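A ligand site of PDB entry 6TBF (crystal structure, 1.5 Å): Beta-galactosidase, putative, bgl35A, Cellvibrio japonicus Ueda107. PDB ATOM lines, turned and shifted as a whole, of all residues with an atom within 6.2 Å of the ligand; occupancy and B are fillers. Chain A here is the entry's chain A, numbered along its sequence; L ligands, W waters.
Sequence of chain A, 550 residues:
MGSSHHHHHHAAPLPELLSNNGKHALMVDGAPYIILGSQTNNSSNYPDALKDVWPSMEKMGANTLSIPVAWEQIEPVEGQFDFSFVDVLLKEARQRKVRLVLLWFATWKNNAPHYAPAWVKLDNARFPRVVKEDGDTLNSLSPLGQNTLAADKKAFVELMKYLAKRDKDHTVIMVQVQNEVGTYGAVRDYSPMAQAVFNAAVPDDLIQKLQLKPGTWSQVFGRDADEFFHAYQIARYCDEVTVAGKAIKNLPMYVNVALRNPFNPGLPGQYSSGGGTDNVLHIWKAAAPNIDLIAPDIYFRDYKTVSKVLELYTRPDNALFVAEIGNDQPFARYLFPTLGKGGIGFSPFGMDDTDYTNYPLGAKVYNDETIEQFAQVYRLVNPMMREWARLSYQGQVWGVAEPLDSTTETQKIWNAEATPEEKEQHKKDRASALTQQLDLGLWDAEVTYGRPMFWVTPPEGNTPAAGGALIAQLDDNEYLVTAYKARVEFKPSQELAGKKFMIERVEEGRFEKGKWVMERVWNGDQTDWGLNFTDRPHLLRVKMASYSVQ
O4 of the ligand is in hydrogen-bond range of OE2 of Glu 324, at 2.7 Å. The side-chain carboxylate of Glu 180 is in salt-bridge range of a nitrogen (N1) of the ligand (2.8 Å). O1 of the ligand sits at hydrogen-bond distance from ND2 of Asn 358 (2.9 Å). An oxygen (O3) of the ligand is in hydrogen-bond range of the side-chain amino group of Lys 109, 2.9 Å away. An oxygen (O4) of the ligand sits at hydrogen-bond distance from the side-chain amide nitrogen (ND2) of Asn 179 (3.0 Å). The side-chain amide nitrogen (ND2) of Asn 110 lies within hydrogen-bond range of an oxygen (O2) of the ligand, 3.0 Å away. O3 of the ligand sits at hydrogen-bond distance from ND2 of Asn 42, 3.0 Å away.
The side-chain amide nitrogen (ND2) of Asn 256 lies within hydrogen-bond range of the side-chain carboxylate (OE2) of Glu 324 (3.0 Å). The side-chain carboxylate (OE2) of Glu 180 sits close to the side-chain carboxylate (OD2) of Asp 297, 2.5 Å away. OD1 of Asn 256 lies within hydrogen-bond range of N of Glu 180 (3.0 Å). The side-chain amino group (NZ) of Lys 109 lies within hydrogen-bond range of the side-chain amide oxygen (OD1) of Asn 42 (2.8 Å). The backbone carbonyl oxygen of Asn 179 sits at hydrogen-bond distance from the backbone NH of Asn 110 (2.8 Å). OD1 of Asn 179 sits at hydrogen-bond distance from ND2 of Asn 256 (2.9 Å). OD2 of Asp 297 sits at hydrogen-bond distance from ND2 of Asn 256, 2.8 Å away. The backbone carbonyl oxygen of Leu 361 is in hydrogen-bond range of the guanidinium group of Arg 301, 3.1 Å away.
ND2 of Asn 256 touches O4 of the ligand, 3.8 Å away. Asp 297 touches the ligand (OD2 to O4, 3.5 Å). Tyr 299 touches the ligand. Phe 300 touches the ligand. CZ of Phe 349 touches C3 of the ligand, 3.6 Å away. CD2 of Leu 361 touches C13 of the ligand, at 3.8 Å. 13 residues have an atom within 4 Å of the ligand: Asn 42, Lys 109, Asn 110, Asn 179, Glu 180, Asn 256, Asp 297, Tyr 299, Phe 300, Glu 324, Phe 349, Asn 358 and Leu 361. The nearest printed residue that does not touch the ligand is Phe 105 (4.3 Å).
Water W1 lies within hydrogen-bond range of a nitrogen (N1) of the ligand and the side-chain amide nitrogen (ND2) of Asn 110.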
ATOM      1  N   GLN A  39      24.785 -14.969  15.256  1.00  0.00           N
ATOM      2  CA  GLN A  39      24.823 -16.340  14.728  1.00  0.00           C
ATOM      3  C   GLN A  39      26.165 -16.943  15.087  1.00  0.00           C
ATOM      4  O   GLN A  39      27.219 -16.367  14.965  1.00  0.00           O
ATOM      5  CB  GLN A  39      24.522 -16.402  13.241  1.00  0.00           C
ATOM      6  CG  GLN A  39      24.672 -17.813  12.677  1.00  0.00           C
ATOM      7  CD  GLN A  39      24.219 -18.093  11.259  1.00  0.00           C
ATOM      8  OE1 GLN A  39      24.628 -19.146  10.703  1.00  0.00           O
ATOM      9  NE2 GLN A  39      23.281 -17.322  10.702  1.00  0.00           N
ATOM     10  N   ASN A  42      29.717 -22.361  12.326  1.00  0.00           N
ATOM     11  CA  ASN A  42      29.010 -23.501  11.736  1.00  0.00           C
ATOM     12  C   ASN A  42      29.169 -24.812  12.515  1.00  0.00           C
ATOM     13  O   ASN A  42      28.412 -25.748  12.188  1.00  0.00           O
ATOM     14  CB  ASN A  42      29.522 -23.708  10.327  1.00  0.00           C
ATOM     15  CG  ASN A  42      28.970 -22.833   9.221  1.00  0.00           C
ATOM     16  OD1 ASN A  42      29.546 -22.871   8.130  1.00  0.00           O
ATOM     17  ND2 ASN A  42      27.903 -22.063   9.462  1.00  0.00           N
ATOM     18  N   PHE A 105      19.971 -27.253   8.645  1.00  0.00           N
ATOM     19  CA  PHE A 105      21.027 -27.625   7.709  1.00  0.00           C
ATOM     20  C   PHE A 105      20.745 -29.038   7.203  1.00  0.00           C
ATOM     21  O   PHE A 105      20.918 -29.991   7.960  1.00  0.00           O
ATOM     22  CB  PHE A 105      22.390 -27.536   8.393  1.00  0.00           C
ATOM     23  CG  PHE A 105      23.000 -26.169   8.626  1.00  0.00           C
ATOM     24  CD1 PHE A 105      22.299 -25.000   8.456  1.00  0.00           C
ATOM     25  CD2 PHE A 105      24.318 -26.074   9.066  1.00  0.00           C
ATOM     26  CE1 PHE A 105      22.910 -23.769   8.683  1.00  0.00           C
ATOM     27  CE2 PHE A 105      24.899 -24.838   9.353  1.00  0.00           C
ATOM     28  CZ  PHE A 105      24.189 -23.678   9.138  1.00  0.00           C
ATOM     29  N   LYS A 109      23.382 -27.013   2.445  1.00  0.00           N
ATOM     30  CA  LYS A 109      24.121 -26.065   3.301  1.00  0.00           C
ATOM     31  C   LYS A 109      25.231 -25.574   2.385  1.00  0.00           C
ATOM     32  O   LYS A 109      26.120 -26.328   2.034  1.00  0.00           O
ATOM     33  CB  LYS A 109      24.586 -26.753   4.605  1.00  0.00           C
ATOM     34  CG  LYS A 109      25.060 -25.806   5.705  1.00  0.00           C
ATOM     35  CD  LYS A 109      26.320 -25.039   5.305  1.00  0.00           C
ATOM     36  CE  LYS A 109      26.852 -24.167   6.422  1.00  0.00           C
ATOM     37  NZ  LYS A 109      27.951 -23.326   5.889  1.00  0.00           N
ATOM     38  N   ASN A 110      25.157 -24.318   1.970  1.00  0.00           N
ATOM     39  CA  ASN A 110      26.115 -23.718   1.018  1.00  0.00           C
ATOM     40  C   ASN A 110      26.216 -24.594  -0.227  1.00  0.00           C
ATOM     41  O   ASN A 110      27.306 -24.947  -0.616  1.00  0.00           O
ATOM     42  CB  ASN A 110      27.479 -23.517   1.647  1.00  0.00           C
ATOM     43  CG  ASN A 110      27.502 -22.444   2.724  1.00  0.00           C
ATOM     44  OD1 ASN A 110      26.559 -22.308   3.500  1.00  0.00           O
ATOM     45  ND2 ASN A 110      28.664 -21.884   2.972  1.00  0.00           N
ATOM     46  N   ASN A 179      20.211 -23.883   4.121  1.00  0.00           N
ATOM     47  CA  ASN A 179      21.168 -22.788   4.249  1.00  0.00           C
ATOM     48  C   ASN A 179      21.817 -22.541   2.907  1.00  0.00           C
ATOM     49  O   ASN A 179      22.561 -23.432   2.399  1.00  0.00           O
ATOM     50  CB  ASN A 179      22.204 -23.011   5.346  1.00  0.00           C
ATOM     51  CG  ASN A 179      23.063 -21.805   5.603  1.00  0.00           C
ATOM     52  OD1 ASN A 179      22.650 -20.961   6.384  1.00  0.00           O
ATOM     53  ND2 ASN A 179      24.233 -21.741   4.935  1.00  0.00           N
ATOM     54  N   GLU A 180      21.674 -21.308   2.382  1.00  0.00           N
ATOM     55  CA  GLU A 180      22.305 -20.932   1.083  1.00  0.00           C
ATOM     56  C   GLU A 180      22.144 -22.071   0.050  1.00  0.00           C
ATOM     57  O   GLU A 180      23.140 -22.674  -0.428  1.00  0.00           O
ATOM     58  CB  GLU A 180      23.771 -20.530   1.299  1.00  0.00           C
ATOM     59  CG  GLU A 180      23.866 -19.171   2.002  1.00  0.00           C
ATOM     60  CD  GLU A 180      25.219 -18.480   2.020  1.00  0.00           C
ATOM     61  OE1 GLU A 180      26.236 -19.126   1.754  1.00  0.00           O
ATOM     62  OE2 GLU A 180      25.257 -17.229   2.378  1.00  0.00           O
ATOM     63  N   TYR A 184      26.968 -24.461  -7.042  1.00  0.00           N
ATOM     64  CA  TYR A 184      28.196 -23.871  -7.610  1.00  0.00           C
ATOM     65  C   TYR A 184      28.719 -24.822  -8.673  1.00  0.00           C
ATOM     66  O   TYR A 184      28.739 -26.058  -8.461  1.00  0.00           O
ATOM     67  CB  TYR A 184      29.281 -23.683  -6.552  1.00  0.00           C
ATOM     68  CG  TYR A 184      28.994 -22.618  -5.517  1.00  0.00           C
ATOM     69  CD1 TYR A 184      28.998 -21.282  -5.827  1.00  0.00           C
ATOM     70  CD2 TYR A 184      28.787 -22.958  -4.190  1.00  0.00           C
ATOM     71  CE1 TYR A 184      28.712 -20.319  -4.857  1.00  0.00           C
ATOM     72  CE2 TYR A 184      28.524 -22.008  -3.202  1.00  0.00           C
ATOM     73  CZ  TYR A 184      28.561 -20.679  -3.547  1.00  0.00           C
ATOM     74  OH  TYR A 184      28.350 -19.670  -2.651  1.00  0.00           O
ATOM     75  N   ASN A 256      17.738 -18.179   3.273  1.00  0.00           N
ATOM     76  CA  ASN A 256      18.830 -17.188   3.209  1.00  0.00           C
ATOM     77  C   ASN A 256      19.625 -17.349   1.922  1.00  0.00           C
ATOM     78  O   ASN A 256      20.096 -18.475   1.560  1.00  0.00           O
ATOM     79  CB  ASN A 256      19.754 -17.288   4.420  1.00  0.00           C
ATOM     80  CG  ASN A 256      20.473 -18.605   4.561  1.00  0.00           C
ATOM     81  OD1 ASN A 256      19.931 -19.662   4.236  1.00  0.00           O
ATOM     82  ND2 ASN A 256      21.688 -18.514   5.131  1.00  0.00           N
ATOM     83  N   ALA A 258      22.887 -16.854  -0.601  1.00  0.00           N
ATOM     84  CA  ALA A 258      24.283 -16.611  -1.022  1.00  0.00           C
ATOM     85  C   ALA A 258      24.228 -15.634  -2.213  1.00  0.00           C
ATOM     86  O   ALA A 258      23.987 -16.031  -3.369  1.00  0.00           O
ATOM     87  CB  ALA A 258      24.970 -17.910  -1.372  1.00  0.00           C
ATOM     88  N   LEU A 259      24.349 -14.342  -1.865  1.00  0.00           N
ATOM     89  CA  LEU A 259      24.119 -13.223  -2.778  1.00  0.00           C
ATOM     90  C   LEU A 259      25.047 -13.323  -3.977  1.00  0.00           C
ATOM     91  O   LEU A 259      26.254 -13.585  -3.801  1.00  0.00           O
ATOM     92  CB  LEU A 259      24.405 -11.927  -2.045  1.00  0.00           C
ATOM     93  CG  LEU A 259      23.427 -11.641  -0.877  1.00  0.00           C
ATOM     94  CD1 LEU A 259      23.806 -10.328  -0.235  1.00  0.00           C
ATOM     95  CD2 LEU A 259      21.953 -11.642  -1.326  1.00  0.00           C
ATOM     96  N   ASP A 297      22.321 -12.646   2.860  1.00  0.00           N
ATOM     97  CA  ASP A 297      23.548 -12.932   3.641  1.00  0.00           C
ATOM     98  C   ASP A 297      24.649 -12.001   3.093  1.00  0.00           C
ATOM     99  O   ASP A 297      25.242 -12.257   2.036  1.00  0.00           O
ATOM    100  CB  ASP A 297      23.983 -14.394   3.510  1.00  0.00           C
ATOM    101  CG  ASP A 297      23.013 -15.414   4.044  1.00  0.00           C
ATOM    102  OD1 ASP A 297      22.123 -15.028   4.839  1.00  0.00           O
ATOM    103  OD2 ASP A 297      23.180 -16.657   3.711  1.00  0.00           O
ATOM    104  N   TYR A 299      28.100 -10.091   2.836  1.00  0.00           N
ATOM    105  CA  TYR A 299      29.563 -10.083   3.134  1.00  0.00           C
ATOM    106  C   TYR A 299      30.291  -9.056   2.254  1.00  0.00           C
ATOM    107  O   TYR A 299      31.510  -8.896   2.379  1.00  0.00           O
ATOM    108  CB  TYR A 299      30.129 -11.492   3.024  1.00  0.00           C
ATOM    109  CG  TYR A 299      29.565 -12.423   4.063  1.00  0.00           C
ATOM    110  CD1 TYR A 299      29.992 -12.361   5.382  1.00  0.00           C
ATOM    111  CD2 TYR A 299      28.539 -13.293   3.741  1.00  0.00           C
ATOM    112  CE1 TYR A 299      29.424 -13.173   6.356  1.00  0.00           C
ATOM    113  CE2 TYR A 299      27.982 -14.132   4.719  1.00  0.00           C
ATOM    114  CZ  TYR A 299      28.435 -14.077   6.023  1.00  0.00           C
ATOM    115  OH  TYR A 299      27.930 -14.859   7.033  1.00  0.00           O
ATOM    116  N   PHE A 300      29.536  -8.296   1.454  1.00  0.00           N
ATOM    117  CA  PHE A 300      30.103  -7.125   0.723  1.00  0.00           C
ATOM    118  C   PHE A 300      30.363  -6.040   1.769  1.00  0.00           C
ATOM    119  O   PHE A 300      29.483  -5.792   2.598  1.00  0.00           O
ATOM    120  CB  PHE A 300      29.179  -6.585  -0.364  1.00  0.00           C
ATOM    121  CG  PHE A 300      28.625  -7.621  -1.291  1.00  0.00           C
ATOM    122  CD1 PHE A 300      29.452  -8.373  -2.119  1.00  0.00           C
ATOM    123  CD2 PHE A 300      27.264  -7.870  -1.350  1.00  0.00           C
ATOM    124  CE1 PHE A 300      28.951  -9.332  -2.967  1.00  0.00           C
ATOM    125  CE2 PHE A 300      26.763  -8.849  -2.183  1.00  0.00           C
ATOM    126  CZ  PHE A 300      27.598  -9.543  -3.014  1.00  0.00           C
ATOM    127  N   ARG A 301      31.593  -5.537   1.838  1.00  0.00           N
ATOM    128  CA  ARG A 301      31.946  -4.517   2.875  1.00  0.00           C
ATOM    129  C   ARG A 301      31.604  -3.084   2.470  1.00  0.00           C
ATOM    130  O   ARG A 301      31.377  -2.207   3.416  1.00  0.00           O
ATOM    131  CB  ARG A 301      33.436  -4.529   3.202  1.00  0.00           C
ATOM    132  CG  ARG A 301      33.842  -5.801   3.919  1.00  0.00           C
ATOM    133  CD  ARG A 301      35.169  -6.398   3.481  1.00  0.00           C
ATOM    134  NE  ARG A 301      35.544  -7.504   4.341  1.00  0.00           N
ATOM    135  CZ  ARG A 301      36.053  -7.284   5.547  1.00  0.00           C
ATOM    136  NH1 ARG A 301      36.251  -6.054   5.966  1.00  0.00           N
ATOM    137  NH2 ARG A 301      36.329  -8.286   6.346  1.00  0.00           N
ATOM    138  N   GLU A 324      22.435 -12.887   7.833  1.00  0.00           N
ATOM    139  CA  GLU A 324      23.866 -12.956   8.151  1.00  0.00           C
ATOM    140  C   GLU A 324      24.480 -11.662   7.681  1.00  0.00           C
ATOM    141  O   GLU A 324      24.066 -11.131   6.620  1.00  0.00           O
ATOM    142  CB  GLU A 324      24.657 -14.076   7.426  1.00  0.00           C
ATOM    143  CG  GLU A 324      24.139 -15.426   7.670  1.00  0.00           C
ATOM    144  CD  GLU A 324      24.725 -16.492   6.793  1.00  0.00           C
ATOM    145  OE1 GLU A 324      25.849 -16.290   6.319  1.00  0.00           O
ATOM    146  OE2 GLU A 324      24.107 -17.561   6.669  1.00  0.00           O
ATOM    147  N   PHE A 349      27.445 -12.761  11.754  1.00  0.00           N
ATOM    148  CA  PHE A 349      27.864 -14.181  11.674  1.00  0.00           C
ATOM    149  C   PHE A 349      29.189 -14.393  12.407  1.00  0.00           C
ATOM    150  O   PHE A 349      30.168 -13.696  12.171  1.00  0.00           O
ATOM    151  CB  PHE A 349      28.017 -14.577  10.228  1.00  0.00           C
ATOM    152  CG  PHE A 349      28.376 -16.010  10.022  1.00  0.00           C
ATOM    153  CD1 PHE A 349      29.686 -16.402  10.038  1.00  0.00           C
ATOM    154  CD2 PHE A 349      27.393 -16.977  10.020  1.00  0.00           C
ATOM    155  CE1 PHE A 349      30.030 -17.743   9.958  1.00  0.00           C
ATOM    156  CE2 PHE A 349      27.724 -18.308   9.926  1.00  0.00           C
ATOM    157  CZ  PHE A 349      29.057 -18.681   9.926  1.00  0.00           C
ATOM    158  N   TYR A 356      37.570 -19.821  15.543  1.00  0.00           N
ATOM    159  CA  TYR A 356      37.416 -19.700  14.089  1.00  0.00           C
ATOM    160  C   TYR A 356      37.072 -18.274  13.717  1.00  0.00           C
ATOM    161  O   TYR A 356      36.268 -17.636  14.376  1.00  0.00           O
ATOM    162  CB  TYR A 356      36.315 -20.591  13.556  1.00  0.00           C
ATOM    163  CG  TYR A 356      36.313 -20.681  12.074  1.00  0.00           C
ATOM    164  CD1 TYR A 356      37.153 -21.587  11.410  1.00  0.00           C
ATOM    165  CD2 TYR A 356      35.444 -19.886  11.318  1.00  0.00           C
ATOM    166  CE1 TYR A 356      37.173 -21.616  10.019  1.00  0.00           C
ATOM    167  CE2 TYR A 356      35.444 -19.929   9.935  1.00  0.00           C
ATOM    168  CZ  TYR A 356      36.295 -20.821   9.284  1.00  0.00           C
ATOM    169  OH  TYR A 356      36.311 -20.804   7.915  1.00  0.00           O
ATOM    170  N   ASN A 358      35.985 -16.322   9.833  1.00  0.00           N
ATOM    171  CA  ASN A 358      35.771 -16.470   8.397  1.00  0.00           C
ATOM    172  C   ASN A 358      36.426 -15.306   7.598  1.00  0.00           C
ATOM    173  O   ASN A 358      36.104 -15.176   6.407  1.00  0.00           O
ATOM    174  CB  ASN A 358      34.292 -16.608   8.086  1.00  0.00           C
ATOM    175  CG  ASN A 358      33.470 -15.347   8.247  1.00  0.00           C
ATOM    176  OD1 ASN A 358      33.955 -14.393   8.885  1.00  0.00           O
ATOM    177  ND2 ASN A 358      32.214 -15.440   7.852  1.00  0.00           N
ATOM    178  N   LEU A 361      36.063 -12.785   4.951  1.00  0.00           N
ATOM    179  CA  LEU A 361      34.662 -12.281   4.981  1.00  0.00           C
ATOM    180  C   LEU A 361      34.456 -11.447   6.262  1.00  0.00           C
ATOM    181  O   LEU A 361      33.954 -10.335   6.168  1.00  0.00           O
ATOM    182  CB  LEU A 361      33.702 -13.424   4.939  1.00  0.00           C
ATOM    183  CG  LEU A 361      33.705 -14.290   3.697  1.00  0.00           C
ATOM    184  CD1 LEU A 361      32.460 -15.128   3.709  1.00  0.00           C
ATOM    185  CD2 LEU A 361      33.772 -13.448   2.414  1.00  0.00           C
HETATM  186  C1  LIG L   1      27.792 -18.139   4.715  1.00  0.00           C
HETATM  187  C2  LIG L   1      28.898 -18.177   5.818  1.00  0.00           C
HETATM  188  C3  LIG L   1      28.738 -19.553   6.496  1.00  0.00           C
HETATM  189  C4  LIG L   1      31.927 -11.028  -0.626  1.00  0.00           C
HETATM  190  C5  LIG L   1      30.311 -17.846   5.462  1.00  0.00           C
HETATM  191  C6  LIG L   1      28.837 -17.044   2.698  1.00  0.00           C
HETATM  192  C7  LIG L   1      27.233 -19.612   6.520  1.00  0.00           C
HETATM  193  C8  LIG L   1      26.876 -19.306   5.090  1.00  0.00           C
HETATM  194  N1  LIG L   1      28.364 -18.331   3.307  1.00  0.00           N
HETATM  195  O1  LIG L   1      31.198 -17.832   6.601  1.00  0.00           O
HETATM  196  O2  LIG L   1      29.228 -20.580   5.612  1.00  0.00           O
HETATM  197  O3  LIG L   1      26.721 -20.892   6.964  1.00  0.00           O
HETATM  198  O4  LIG L   1      25.462 -19.058   4.922  1.00  0.00           O
HETATM  199  C9  LIG L   1      29.306 -17.311   1.261  1.00  0.00           C
HETATM  200  C10 LIG L   1      29.668 -15.965   0.612  1.00  0.00           C
HETATM  201  C11 LIG L   1      31.020 -15.882   0.012  1.00  0.00           C
HETATM  202  C12 LIG L   1      31.019 -14.739  -0.992  1.00  0.00           C
HETATM  203  C13 LIG L   1      31.153 -13.365  -0.385  1.00  0.00           C
HETATM  204  C14 LIG L   1      31.923 -12.389  -1.306  1.00  0.00           C
HETATM  205  O   HOH W   1      30.836 -19.811   2.525  1.00  0.00           O
HETATM  206  O   HOH W   2      24.546 -20.473   8.341  1.00  0.00           O
